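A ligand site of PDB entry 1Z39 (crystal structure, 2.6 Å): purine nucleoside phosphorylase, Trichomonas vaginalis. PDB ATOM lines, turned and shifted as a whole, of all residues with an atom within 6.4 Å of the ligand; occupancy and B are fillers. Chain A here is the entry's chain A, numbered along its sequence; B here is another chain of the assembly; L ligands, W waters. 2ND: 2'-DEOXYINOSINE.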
ATOM      1  N   GLY A  20      27.032  -2.564 -29.732  1.00  0.00           N
ATOM      2  CA  GLY A  20      25.983  -2.525 -30.735  1.00  0.00           C
ATOM      3  C   GLY A  20      25.758  -1.157 -31.317  1.00  0.00           C
ATOM      4  O   GLY A  20      25.668  -0.993 -32.531  1.00  0.00           O
ATOM      5  N   ASP A  21      25.659  -0.156 -30.445  1.00  0.00           N
ATOM      6  CA  ASP A  21      25.422   1.222 -30.843  1.00  0.00           C
ATOM      7  C   ASP A  21      26.635   1.886 -31.508  1.00  0.00           C
ATOM      8  O   ASP A  21      27.662   2.130 -30.866  1.00  0.00           O
ATOM      9  CB  ASP A  21      24.995   2.034 -29.626  1.00  0.00           C
ATOM     10  CG  ASP A  21      24.556   3.440 -29.979  1.00  0.00           C
ATOM     11  OD1 ASP A  21      24.907   3.910 -31.082  1.00  0.00           O
ATOM     12  OD2 ASP A  21      23.871   4.073 -29.148  1.00  0.00           O
ATOM     13  N   HIS A  62      28.642  -3.137 -34.011  1.00  0.00           N
ATOM     14  CA  HIS A  62      28.386  -4.457 -34.580  1.00  0.00           C
ATOM     15  C   HIS A  62      26.912  -4.746 -34.768  1.00  0.00           C
ATOM     16  O   HIS A  62      26.532  -5.893 -35.000  1.00  0.00           O
ATOM     17  CB  HIS A  62      29.027  -5.556 -33.705  1.00  0.00           C
ATOM     18  CG  HIS A  62      28.498  -5.621 -32.310  1.00  0.00           C
ATOM     19  ND1 HIS A  62      27.159  -5.765 -32.016  1.00  0.00           N
ATOM     20  CD2 HIS A  62      29.141  -5.584 -31.113  1.00  0.00           C
ATOM     21  CE1 HIS A  62      27.006  -5.823 -30.704  1.00  0.00           C
ATOM     22  NE2 HIS A  62      28.191  -5.709 -30.133  1.00  0.00           N
ATOM     23  N   GLY A  63      26.081  -3.699 -34.679  1.00  0.00           N
ATOM     24  CA  GLY A  63      24.644  -3.877 -34.850  1.00  0.00           C
ATOM     25  C   GLY A  63      24.064  -4.797 -33.787  1.00  0.00           C
ATOM     26  O   GLY A  63      24.781  -5.266 -32.916  1.00  0.00           O
ATOM     27  N   MET A  64      22.766  -5.049 -33.853  1.00  0.00           N
ATOM     28  CA  MET A  64      22.131  -5.917 -32.865  1.00  0.00           C
ATOM     29  C   MET A  64      21.811  -7.286 -33.443  1.00  0.00           C
ATOM     30  O   MET A  64      21.335  -7.391 -34.561  1.00  0.00           O
ATOM     31  CB  MET A  64      20.842  -5.286 -32.349  1.00  0.00           C
ATOM     32  CG  MET A  64      21.007  -3.889 -31.799  1.00  0.00           C
ATOM     33  SD  MET A  64      19.426  -3.229 -31.258  1.00  0.00           S
ATOM     34  CE  MET A  64      18.604  -2.964 -32.851  1.00  0.00           C
ATOM     35  N   GLY A  65      22.083  -8.333 -32.659  1.00  0.00           N
ATOM     36  CA  GLY A  65      21.793  -9.687 -33.098  1.00  0.00           C
ATOM     37  C   GLY A  65      22.970 -10.530 -33.552  1.00  0.00           C
ATOM     38  O   GLY A  65      23.951 -10.013 -34.091  1.00  0.00           O
ATOM     39  N   ARG A  87      33.481  -7.716 -26.721  1.00  0.00           N
ATOM     40  CA  ARG A  87      32.188  -7.048 -26.842  1.00  0.00           C
ATOM     41  C   ARG A  87      31.942  -6.287 -25.540  1.00  0.00           C
ATOM     42  O   ARG A  87      31.992  -6.838 -24.443  1.00  0.00           O
ATOM     43  CB  ARG A  87      31.057  -8.059 -27.085  1.00  0.00           C
ATOM     44  CG  ARG A  87      29.684  -7.395 -27.123  1.00  0.00           C
ATOM     45  CD  ARG A  87      28.560  -8.400 -27.178  1.00  0.00           C
ATOM     46  NE  ARG A  87      27.377  -7.931 -26.453  1.00  0.00           N
ATOM     47  CZ  ARG A  87      26.774  -6.765 -26.668  1.00  0.00           C
ATOM     48  NH1 ARG A  87      27.240  -5.928 -27.589  1.00  0.00           N
ATOM     49  NH2 ARG A  87      25.709  -6.421 -25.963  1.00  0.00           N
ATOM     50  N   THR A  90      25.626  -3.130 -23.130  1.00  0.00           N
ATOM     51  CA  THR A  90      24.575  -3.230 -22.133  1.00  0.00           C
ATOM     52  C   THR A  90      23.879  -4.569 -22.251  1.00  0.00           C
ATOM     53  O   THR A  90      24.036  -5.281 -23.241  1.00  0.00           O
ATOM     54  CB  THR A  90      23.526  -2.139 -22.330  1.00  0.00           C
ATOM     55  OG1 THR A  90      22.875  -2.337 -23.597  1.00  0.00           O
ATOM     56  CG2 THR A  90      24.177  -0.762 -22.305  1.00  0.00           C
ATOM     57  N   CYS A  91      23.106  -4.903 -21.225  1.00  0.00           N
ATOM     58  CA  CYS A  91      22.382  -6.163 -21.194  1.00  0.00           C
ATOM     59  C   CYS A  91      21.222  -6.048 -20.212  1.00  0.00           C
ATOM     60  O   CYS A  91      21.115  -5.062 -19.483  1.00  0.00           O
ATOM     61  CB  CYS A  91      23.325  -7.294 -20.782  1.00  0.00           C
ATOM     62  SG  CYS A  91      24.082  -7.059 -19.136  1.00  0.00           S
ATOM     63  N   GLY A  92      20.350  -7.053 -20.208  1.00  0.00           N
ATOM     64  CA  GLY A  92      19.216  -7.059 -19.304  1.00  0.00           C
ATOM     65  C   GLY A  92      19.366  -8.134 -18.252  1.00  0.00           C
ATOM     66  O   GLY A  92      19.508  -9.318 -18.567  1.00  0.00           O
ATOM     67  N   ALA A  93      19.344  -7.731 -16.981  1.00  0.00           N
ATOM     68  CA  ALA A  93      19.487  -8.680 -15.879  1.00  0.00           C
ATOM     69  C   ALA A  93      18.367  -9.700 -15.865  1.00  0.00           C
ATOM     70  O   ALA A  93      17.230  -9.411 -16.227  1.00  0.00           O
ATOM     71  CB  ALA A  93      19.524  -7.938 -14.545  1.00  0.00           C
ATOM     72  N   PHE A 154      23.083 -14.804 -21.926  1.00  0.00           N
ATOM     73  CA  PHE A 154      22.149 -15.413 -22.850  1.00  0.00           C
ATOM     74  C   PHE A 154      21.957 -14.466 -24.025  1.00  0.00           C
ATOM     75  O   PHE A 154      21.589 -13.304 -23.827  1.00  0.00           O
ATOM     76  CB  PHE A 154      20.793 -15.672 -22.192  1.00  0.00           C
ATOM     77  CG  PHE A 154      19.815 -16.381 -23.077  1.00  0.00           C
ATOM     78  CD1 PHE A 154      19.934 -17.758 -23.320  1.00  0.00           C
ATOM     79  CD2 PHE A 154      18.771 -15.690 -23.693  1.00  0.00           C
ATOM     80  CE1 PHE A 154      19.032 -18.416 -24.151  1.00  0.00           C
ATOM     81  CE2 PHE A 154      17.873 -16.335 -24.526  1.00  0.00           C
ATOM     82  CZ  PHE A 154      18.000 -17.712 -24.753  1.00  0.00           C
ATOM     83  N   THR A 156      19.753 -13.681 -27.009  1.00  0.00           N
ATOM     84  CA  THR A 156      18.440 -13.958 -27.580  1.00  0.00           C
ATOM     85  C   THR A 156      18.294 -13.402 -28.996  1.00  0.00           C
ATOM     86  O   THR A 156      18.938 -12.420 -29.378  1.00  0.00           O
ATOM     87  CB  THR A 156      17.302 -13.337 -26.714  1.00  0.00           C
ATOM     88  OG1 THR A 156      16.030 -13.684 -27.267  1.00  0.00           O
ATOM     89  CG2 THR A 156      17.413 -11.809 -26.686  1.00  0.00           C
ATOM     90  N   LEU A 158      15.193 -12.857 -29.909  1.00  0.00           N
ATOM     91  CA  LEU A 158      13.962 -12.107 -29.687  1.00  0.00           C
ATOM     92  C   LEU A 158      14.012 -11.123 -28.521  1.00  0.00           C
ATOM     93  O   LEU A 158      13.740 -11.508 -27.377  1.00  0.00           O
ATOM     94  CB  LEU A 158      12.801 -13.091 -29.468  1.00  0.00           C
ATOM     95  CG  LEU A 158      11.937 -13.671 -30.603  1.00  0.00           C
ATOM     96  CD1 LEU A 158      12.365 -13.118 -31.940  1.00  0.00           C
ATOM     97  CD2 LEU A 158      12.009 -15.187 -30.577  1.00  0.00           C
ATOM     98  N   PHE A 159      14.342  -9.858 -28.794  1.00  0.00           N
ATOM     99  CA  PHE A 159      14.364  -8.863 -27.736  1.00  0.00           C
ATOM    100  C   PHE A 159      12.979  -8.904 -27.060  1.00  0.00           C
ATOM    101  O   PHE A 159      12.879  -8.898 -25.823  1.00  0.00           O
ATOM    102  CB  PHE A 159      14.617  -7.471 -28.309  1.00  0.00           C
ATOM    103  CG  PHE A 159      14.609  -6.374 -27.280  1.00  0.00           C
ATOM    104  CD1 PHE A 159      15.790  -5.972 -26.669  1.00  0.00           C
ATOM    105  CD2 PHE A 159      13.410  -5.778 -26.897  1.00  0.00           C
ATOM    106  CE1 PHE A 159      15.774  -4.975 -25.690  1.00  0.00           C
ATOM    107  CE2 PHE A 159      13.381  -4.792 -25.917  1.00  0.00           C
ATOM    108  CZ  PHE A 159      14.574  -4.387 -25.313  1.00  0.00           C
ATOM    109  N   VAL A 178      20.981 -10.837 -20.294  1.00  0.00           N
ATOM    110  CA  VAL A 178      20.637 -11.117 -21.683  1.00  0.00           C
ATOM    111  C   VAL A 178      21.085 -10.020 -22.642  1.00  0.00           C
ATOM    112  O   VAL A 178      20.862  -8.836 -22.397  1.00  0.00           O
ATOM    113  CB  VAL A 178      19.112 -11.270 -21.856  1.00  0.00           C
ATOM    114  CG1 VAL A 178      18.761 -11.448 -23.342  1.00  0.00           C
ATOM    115  CG2 VAL A 178      18.621 -12.440 -21.058  1.00  0.00           C
ATOM    116  N   GLU A 179      21.722 -10.433 -23.732  1.00  0.00           N
ATOM    117  CA  GLU A 179      22.132  -9.505 -24.778  1.00  0.00           C
ATOM    118  C   GLU A 179      21.828 -10.184 -26.118  1.00  0.00           C
ATOM    119  O   GLU A 179      20.958 -11.062 -26.162  1.00  0.00           O
ATOM    120  CB  GLU A 179      23.610  -9.084 -24.648  1.00  0.00           C
ATOM    121  CG  GLU A 179      24.607 -10.152 -24.260  1.00  0.00           C
ATOM    122  CD  GLU A 179      24.887 -11.132 -25.384  1.00  0.00           C
ATOM    123  OE1 GLU A 179      24.214 -12.180 -25.436  1.00  0.00           O
ATOM    124  OE2 GLU A 179      25.769 -10.836 -26.213  1.00  0.00           O
ATOM    125  N   MET A 180      22.513  -9.824 -27.197  1.00  0.00           N
ATOM    126  CA  MET A 180      22.163 -10.438 -28.481  1.00  0.00           C
ATOM    127  C   MET A 180      23.315 -10.755 -29.431  1.00  0.00           C
ATOM    128  O   MET A 180      23.112 -10.772 -30.639  1.00  0.00           O
ATOM    129  CB  MET A 180      21.155  -9.532 -29.199  1.00  0.00           C
ATOM    130  CG  MET A 180      19.903  -9.254 -28.381  1.00  0.00           C
ATOM    131  SD  MET A 180      18.698  -8.141 -29.155  1.00  0.00           S
ATOM    132  CE  MET A 180      18.040  -9.153 -30.486  1.00  0.00           C
ATOM    133  N   GLU A 181      24.500 -11.024 -28.906  1.00  0.00           N
ATOM    134  CA  GLU A 181      25.636 -11.267 -29.783  1.00  0.00           C
ATOM    135  C   GLU A 181      26.685 -12.291 -29.329  1.00  0.00           C
ATOM    136  O   GLU A 181      27.221 -13.034 -30.142  1.00  0.00           O
ATOM    137  CB  GLU A 181      26.342  -9.942 -30.060  1.00  0.00           C
ATOM    138  CG  GLU A 181      25.484  -8.892 -30.757  1.00  0.00           C
ATOM    139  CD  GLU A 181      24.524  -8.152 -29.826  1.00  0.00           C
ATOM    140  OE1 GLU A 181      23.619  -7.459 -30.335  1.00  0.00           O
ATOM    141  OE2 GLU A 181      24.685  -8.237 -28.594  1.00  0.00           O
ATOM    142  N   SER A 203      21.572  -2.471 -17.962  1.00  0.00           N
ATOM    143  CA  SER A 203      20.819  -1.249 -18.143  1.00  0.00           C
ATOM    144  C   SER A 203      19.384  -1.354 -17.623  1.00  0.00           C
ATOM    145  O   SER A 203      18.679  -0.342 -17.524  1.00  0.00           O
ATOM    146  CB  SER A 203      20.812  -0.844 -19.615  1.00  0.00           C
ATOM    147  OG  SER A 203      20.442  -1.938 -20.426  1.00  0.00           O
ATOM    148  N   ASP A 204      18.962  -2.571 -17.299  1.00  0.00           N
ATOM    149  CA  ASP A 204      17.616  -2.775 -16.779  1.00  0.00           C
ATOM    150  C   ASP A 204      17.419  -4.242 -16.381  1.00  0.00           C
ATOM    151  O   ASP A 204      18.181  -5.115 -16.799  1.00  0.00           O
ATOM    152  CB  ASP A 204      16.581  -2.368 -17.833  1.00  0.00           C
ATOM    153  CG  ASP A 204      15.163  -2.348 -17.280  1.00  0.00           C
ATOM    154  OD1 ASP A 204      14.943  -1.789 -16.180  1.00  0.00           O
ATOM    155  OD2 ASP A 204      14.277  -2.882 -17.963  1.00  0.00           O
ATOM    156  N   ILE A 206      14.795  -7.551 -16.299  1.00  0.00           N
ATOM    157  CA  ILE A 206      13.607  -8.026 -16.978  1.00  0.00           C
ATOM    158  C   ILE A 206      12.570  -8.691 -16.076  1.00  0.00           C
ATOM    159  O   ILE A 206      11.417  -8.839 -16.478  1.00  0.00           O
ATOM    160  CB  ILE A 206      13.961  -9.023 -18.125  1.00  0.00           C
ATOM    161  CG1 ILE A 206      14.318 -10.388 -17.567  1.00  0.00           C
ATOM    162  CG2 ILE A 206      15.121  -8.474 -18.946  1.00  0.00           C
ATOM    163  CD1 ILE A 206      14.559 -11.431 -18.635  1.00  0.00           C
ATOM    164  N   PRO B   3      13.249   1.645 -26.297  1.00  0.00           N
ATOM    165  CA  PRO B   3      14.698   1.534 -26.099  1.00  0.00           C
ATOM    166  C   PRO B   3      15.499   1.793 -27.376  1.00  0.00           C
ATOM    167  O   PRO B   3      16.701   2.034 -27.316  1.00  0.00           O
ATOM    168  CB  PRO B   3      14.872   0.093 -25.629  1.00  0.00           C
ATOM    169  CG  PRO B   3      13.576  -0.185 -24.922  1.00  0.00           C
ATOM    170  CD  PRO B   3      12.562   0.422 -25.860  1.00  0.00           C
ATOM    171  N   HIS B   4      14.837   1.752 -28.533  1.00  0.00           N
ATOM    172  CA  HIS B   4      15.526   1.947 -29.809  1.00  0.00           C
ATOM    173  C   HIS B   4      14.962   3.079 -30.657  1.00  0.00           C
ATOM    174  O   HIS B   4      15.394   3.284 -31.791  1.00  0.00           O
ATOM    175  CB  HIS B   4      15.479   0.648 -30.618  1.00  0.00           C
ATOM    176  CG  HIS B   4      15.793  -0.578 -29.807  1.00  0.00           C
ATOM    177  ND1 HIS B   4      14.852  -1.220 -29.046  1.00  0.00           N
ATOM    178  CD2 HIS B   4      16.958  -1.244 -29.618  1.00  0.00           C
ATOM    179  CE1 HIS B   4      15.416  -2.228 -28.406  1.00  0.00           C
ATOM    180  NE2 HIS B   4      16.692  -2.271 -28.745  1.00  0.00           N
ATOM    181  N   ARG B  43      21.040   5.067 -31.978  1.00  0.00           N
ATOM    182  CA  ARG B  43      21.952   4.105 -32.583  1.00  0.00           C
ATOM    183  C   ARG B  43      22.241   4.448 -34.037  1.00  0.00           C
ATOM    184  O   ARG B  43      22.527   3.564 -34.842  1.00  0.00           O
ATOM    185  CB  ARG B  43      21.374   2.691 -32.490  1.00  0.00           C
ATOM    186  CG  ARG B  43      21.256   2.176 -31.069  1.00  0.00           C
ATOM    187  CD  ARG B  43      20.327   0.983 -30.977  1.00  0.00           C
ATOM    188  NE  ARG B  43      20.346   0.411 -29.636  1.00  0.00           N
ATOM    189  CZ  ARG B  43      21.278  -0.433 -29.200  1.00  0.00           C
ATOM    190  NH1 ARG B  43      22.257  -0.815 -30.005  1.00  0.00           N
ATOM    191  NH2 ARG B  43      21.230  -0.894 -27.959  1.00  0.00           N
ATOM    192  N   ILE B  71      13.115  -6.141 -33.841  1.00  0.00           N
ATOM    193  CA  ILE B  71      12.993  -5.143 -32.798  1.00  0.00           C
ATOM    194  C   ILE B  71      12.277  -3.905 -33.367  1.00  0.00           C
ATOM    195  O   ILE B  71      11.273  -3.441 -32.810  1.00  0.00           O
ATOM    196  CB  ILE B  71      14.377  -4.724 -32.290  1.00  0.00           C
ATOM    197  CG1 ILE B  71      14.976  -5.852 -31.452  1.00  0.00           C
ATOM    198  CG2 ILE B  71      14.269  -3.427 -31.504  1.00  0.00           C
ATOM    199  CD1 ILE B  71      16.428  -5.640 -31.096  1.00  0.00           C
HETATM  200  O6  2ND L   1      17.378  -6.796 -21.917  1.00  0.00           O
HETATM  201  C6  2ND L   1      17.920  -6.972 -23.002  1.00  0.00           C
HETATM  202  N1  2ND L   1      17.472  -7.997 -23.858  1.00  0.00           N
HETATM  203  C2  2ND L   1      18.120  -8.191 -25.084  1.00  0.00           C
HETATM  204  N3  2ND L   1      19.131  -7.423 -25.427  1.00  0.00           N
HETATM  205  C4  2ND L   1      19.584  -6.431 -24.645  1.00  0.00           C
HETATM  206  C5  2ND L   1      18.990  -6.185 -23.412  1.00  0.00           C
HETATM  207  N7  2ND L   1      19.617  -5.146 -22.865  1.00  0.00           N
HETATM  208  C8  2ND L   1      20.571  -4.755 -23.713  1.00  0.00           C
HETATM  209  N9  2ND L   1      20.549  -5.538 -24.799  1.00  0.00           N
HETATM  210  C1' 2ND L   1      21.435  -5.358 -25.970  1.00  0.00           C
HETATM  211  O4' 2ND L   1      21.140  -4.122 -26.650  1.00  0.00           O
HETATM  212  C2' 2ND L   1      21.301  -6.481 -27.009  1.00  0.00           C
HETATM  213  C3' 2ND L   1      21.310  -5.714 -28.328  1.00  0.00           C
HETATM  214  O3' 2ND L   1      22.647  -5.419 -28.734  1.00  0.00           O
HETATM  215  C4' 2ND L   1      20.551  -4.442 -27.917  1.00  0.00           C
HETATM  216  C5' 2ND L   1      19.045  -4.672 -27.749  1.00  0.00           C
HETATM  217  O5' 2ND L   1      18.466  -3.506 -27.164  1.00  0.00           O
HETATM  218  O   HOH W   1      14.841 -10.003 -23.996  1.00  0.00           O
HETATM  219  O   HOH W   2      18.917  -1.548 -25.185  1.00  0.00           O
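The backbone NH (N) of Gly 92 sits at hydrogen-bond distance from a nitrogen (N7) of the ligand (3.4 Å).
The guanidinium group of Arg 43 of chain B lies within hydrogen-bond range of an oxygen (O4') of the ligand (3.5 Å).
A ring nitrogen (NE2) of His 4 of chain B sits at hydrogen-bond distance from an oxygen (O5') of the ligand, 2.7 Å away.
OE1 of Glu 181 sits at hydrogen-bond distance from O3' of the ligand (2.8 Å).
The side-chain carboxylate (OE1) of Glu 181 sits at hydrogen-bond distance from the backbone NH (N) of Gly 65 (2.9 Å).
N of Ser 203 sits at hydrogen-bond distance from O of Cys 91.
O of Met 180 sits close to N of Gly 65 (3.3 Å).
O of Thr 90 sits at hydrogen-bond distance from NH2 of Arg 87 (3.4 Å).
N of Glu 181 sits at hydrogen-bond distance from OE2 of Glu 179 (3.0 Å).
The backbone carbonyl oxygen (O) of Phe 154 is in hydrogen-bond range of the backbone NH (N) of Glu 179, 2.9 Å away.
O of Glu 179 is in hydrogen-bond range of N of Thr 156, at 3.0 Å.
The side-chain carboxylate (OE2) of Glu 181 is in salt-bridge range of the guanidinium group (NH2) of Arg 87 (3.4 Å).
Residues that only touch the ligand: Met 64, Thr 90, Cys 91, Phe 159, Val 178, Glu 179 and Met 180.
Within 4 Å of the ligand: Met 64, Thr 90, Cys 91, Gly 92, Phe 159, Val 178, Glu 179, Met 180, Glu 181, His 4 of chain B and Arg 43 of chain B.
Water W1 lies within hydrogen-bond range of the backbone carbonyl oxygen (O) of Phe 159 (2.9 Å) and a nitrogen (N1) of the ligand (3.3 Å).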
